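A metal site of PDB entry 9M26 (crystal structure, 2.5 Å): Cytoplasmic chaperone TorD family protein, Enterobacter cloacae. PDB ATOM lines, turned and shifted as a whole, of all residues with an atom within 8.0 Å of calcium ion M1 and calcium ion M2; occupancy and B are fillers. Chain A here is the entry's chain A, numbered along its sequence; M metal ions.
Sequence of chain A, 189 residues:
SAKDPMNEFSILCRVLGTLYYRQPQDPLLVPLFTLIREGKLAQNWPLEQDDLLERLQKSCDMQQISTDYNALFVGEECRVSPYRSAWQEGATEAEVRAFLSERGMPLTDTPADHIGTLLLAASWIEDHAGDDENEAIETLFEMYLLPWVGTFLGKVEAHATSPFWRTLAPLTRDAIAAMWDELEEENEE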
ATOM      1  N   LYS A   3      32.596 -10.478  -6.194  1.00  0.00           N
ATOM      2  CA  LYS A   3      31.785 -11.652  -5.930  1.00  0.00           C
ATOM      3  C   LYS A   3      30.306 -11.265  -5.961  1.00  0.00           C
ATOM      4  O   LYS A   3      29.933 -10.168  -5.551  1.00  0.00           O
ATOM      5  CB  LYS A   3      32.164 -12.273  -4.581  1.00  0.00           C
ATOM      6  CG  LYS A   3      32.692 -13.709  -4.639  1.00  0.00           C
ATOM      7  CD  LYS A   3      33.318 -14.187  -3.304  1.00  0.00           C
ATOM      8  CE  LYS A   3      32.306 -14.807  -2.340  1.00  0.00           C
ATOM      9  NZ  LYS A   3      31.795 -16.138  -2.781  1.00  0.00           N
ATOM     10  N   ALA A 177      23.709 -14.233   9.498  1.00  0.00           N
ATOM     11  CA  ALA A 177      25.000 -13.651   9.841  1.00  0.00           C
ATOM     12  C   ALA A 177      26.081 -14.106   8.876  1.00  0.00           C
ATOM     13  O   ALA A 177      26.991 -13.343   8.547  1.00  0.00           O
ATOM     14  CB  ALA A 177      25.372 -13.997  11.284  1.00  0.00           C
ATOM     15  N   ALA A 178      26.003 -15.357   8.420  1.00  0.00           N
ATOM     16  CA  ALA A 178      26.994 -15.878   7.492  1.00  0.00           C
ATOM     17  C   ALA A 178      26.838 -15.246   6.115  1.00  0.00           C
ATOM     18  O   ALA A 178      27.833 -14.966   5.430  1.00  0.00           O
ATOM     19  CB  ALA A 178      26.889 -17.395   7.410  1.00  0.00           C
ATOM     20  N   MET A 179      25.593 -15.016   5.684  1.00  0.00           N
ATOM     21  CA  MET A 179      25.375 -14.331   4.413  1.00  0.00           C
ATOM     22  C   MET A 179      25.848 -12.898   4.477  1.00  0.00           C
ATOM     23  O   MET A 179      26.512 -12.420   3.544  1.00  0.00           O
ATOM     24  CB  MET A 179      23.898 -14.363   4.051  1.00  0.00           C
ATOM     25  CG  MET A 179      23.380 -15.698   3.582  1.00  0.00           C
ATOM     26  SD  MET A 179      21.678 -15.538   3.004  1.00  0.00           S
ATOM     27  CE  MET A 179      20.846 -14.952   4.477  1.00  0.00           C
ATOM     28  N   TRP A 180      25.538 -12.211   5.572  1.00  0.00           N
ATOM     29  CA  TRP A 180      25.879 -10.795   5.714  1.00  0.00           C
ATOM     30  C   TRP A 180      27.388 -10.571   5.675  1.00  0.00           C
ATOM     31  O   TRP A 180      27.860  -9.596   5.075  1.00  0.00           O
ATOM     32  CB  TRP A 180      25.280 -10.226   6.993  1.00  0.00           C
ATOM     33  CG  TRP A 180      25.512  -8.761   7.129  1.00  0.00           C
ATOM     34  CD1 TRP A 180      26.128  -8.107   8.170  1.00  0.00           C
ATOM     35  CD2 TRP A 180      25.192  -7.748   6.165  1.00  0.00           C
ATOM     36  NE1 TRP A 180      26.154  -6.749   7.929  1.00  0.00           N
ATOM     37  CE2 TRP A 180      25.591  -6.503   6.698  1.00  0.00           C
ATOM     38  CE3 TRP A 180      24.571  -7.768   4.906  1.00  0.00           C
ATOM     39  CZ2 TRP A 180      25.393  -5.304   6.027  1.00  0.00           C
ATOM     40  CZ3 TRP A 180      24.394  -6.568   4.229  1.00  0.00           C
ATOM     41  CH2 TRP A 180      24.798  -5.362   4.795  1.00  0.00           C
ATOM     42  N   ASP A 181      28.152 -11.460   6.320  1.00  0.00           N
ATOM     43  CA  ASP A 181      29.606 -11.329   6.271  1.00  0.00           C
ATOM     44  C   ASP A 181      30.117 -11.399   4.843  1.00  0.00           C
ATOM     45  O   ASP A 181      31.018 -10.637   4.461  1.00  0.00           O
ATOM     46  CB  ASP A 181      30.267 -12.424   7.117  1.00  0.00           C
ATOM     47  CG  ASP A 181      31.777 -12.487   6.921  1.00  0.00           C
ATOM     48  OD1 ASP A 181      32.521 -11.672   7.535  1.00  0.00           O
ATOM     49  OD2 ASP A 181      32.210 -13.357   6.134  1.00  0.00           O
ATOM     50  N   GLU A 182      29.531 -12.262   4.018  1.00  0.00           N
ATOM     51  CA  GLU A 182      30.018 -12.419   2.643  1.00  0.00           C
ATOM     52  C   GLU A 182      29.627 -11.220   1.768  1.00  0.00           C
ATOM     53  O   GLU A 182      30.408 -10.777   0.920  1.00  0.00           O
ATOM     54  CB  GLU A 182      29.462 -13.713   2.070  1.00  0.00           C
ATOM     55  CG  GLU A 182      30.476 -14.528   1.299  1.00  0.00           C
ATOM     56  CD  GLU A 182      31.707 -14.855   2.140  1.00  0.00           C
ATOM     57  OE1 GLU A 182      32.810 -14.916   1.558  1.00  0.00           O
ATOM     58  OE2 GLU A 182      31.583 -15.013   3.375  1.00  0.00           O
ATOM     59  N   LEU A 183      28.406 -10.696   1.960  1.00  0.00           N
ATOM     60  CA  LEU A 183      27.963  -9.493   1.254  1.00  0.00           C
ATOM     61  C   LEU A 183      28.774  -8.268   1.663  1.00  0.00           C
ATOM     62  O   LEU A 183      29.234  -7.497   0.817  1.00  0.00           O
ATOM     63  CB  LEU A 183      26.466  -9.262   1.485  1.00  0.00           C
ATOM     64  CG  LEU A 183      25.553 -10.415   1.047  1.00  0.00           C
ATOM     65  CD1 LEU A 183      24.199 -10.361   1.749  1.00  0.00           C
ATOM     66  CD2 LEU A 183      25.381 -10.422  -0.454  1.00  0.00           C
ATOM     67  N   GLU A 184      28.932  -8.057   2.979  1.00  0.00           N
ATOM     68  CA  GLU A 184      29.674  -6.891   3.453  1.00  0.00           C
ATOM     69  C   GLU A 184      31.109  -6.914   2.958  1.00  0.00           C
ATOM     70  O   GLU A 184      31.677  -5.843   2.687  1.00  0.00           O
ATOM     71  CB  GLU A 184      29.662  -6.804   4.969  1.00  0.00           C
ATOM     72  CG  GLU A 184      28.554  -5.949   5.529  1.00  0.00           C
ATOM     73  CD  GLU A 184      28.575  -4.508   5.035  1.00  0.00           C
ATOM     74  OE1 GLU A 184      28.079  -4.248   3.920  1.00  0.00           O
ATOM     75  OE2 GLU A 184      29.062  -3.624   5.771  1.00  0.00           O
ATOM     76  N   GLU A 185      31.711  -8.105   2.808  1.00  0.00           N
ATOM     77  CA  GLU A 185      33.082  -8.161   2.331  1.00  0.00           C
ATOM     78  C   GLU A 185      33.184  -7.643   0.900  1.00  0.00           C
ATOM     79  O   GLU A 185      34.230  -7.139   0.493  1.00  0.00           O
ATOM     80  CB  GLU A 185      33.628  -9.590   2.396  1.00  0.00           C
ATOM     81  CG  GLU A 185      34.035 -10.070   3.780  1.00  0.00           C
ATOM     82  CD  GLU A 185      34.116 -11.590   3.874  1.00  0.00           C
ATOM     83  OE1 GLU A 185      33.619 -12.284   2.968  1.00  0.00           O
ATOM     84  OE2 GLU A 185      34.704 -12.096   4.854  1.00  0.00           O
ATOM     85  N   GLU A 186      32.087  -7.726   0.149  1.00  0.00           N
ATOM     86  CA  GLU A 186      32.031  -7.156  -1.189  1.00  0.00           C
ATOM     87  C   GLU A 186      31.504  -5.731  -1.182  1.00  0.00           C
ATOM     88  O   GLU A 186      31.923  -4.918  -2.020  1.00  0.00           O
ATOM     89  CB  GLU A 186      31.143  -8.025  -2.095  1.00  0.00           C
ATOM     90  CG  GLU A 186      31.621  -9.477  -2.221  1.00  0.00           C
ATOM     91  CD  GLU A 186      33.118  -9.585  -2.508  1.00  0.00           C
ATOM     92  OE1 GLU A 186      33.576  -9.185  -3.600  1.00  0.00           O
ATOM     93  OE2 GLU A 186      33.853 -10.050  -1.617  1.00  0.00           O
HETATM   94 CA    CA M   1      33.899 -14.521   4.911  1.00  0.00          CA
HETATM   95 CA    CA M   2      35.205 -11.597   7.336  1.00  0.00          CA
HETATM   96 CA    CA M   3      38.455  -8.194   1.524  1.00  0.00          CA
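Calcium ion M1 is bound by OD2 of Asp 181 (2.4 Å), OE2 of Glu 185 (2.6 Å) and OE2 of Glu 182 (2.8 Å).
Slightly farther from calcium ion M1 lies OE1 of Glu 185 (3.0 Å).
Calcium ion M2 is bound by OE2 of Glu 185 (2.6 Å) and OD1 of Asp 181 (2.7 Å).
Calcium ion M2 has two donor atoms within binding distance.
Of the 11 residues printed, 3 come within 4 Å of calcium ion M1.
The nearest printed residue that does not touch calcium ion M1 is Ala 178 (6.1 Å).
Two residues have an atom within 4 Å of calcium ion M2: Asp 181 and Glu 185.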
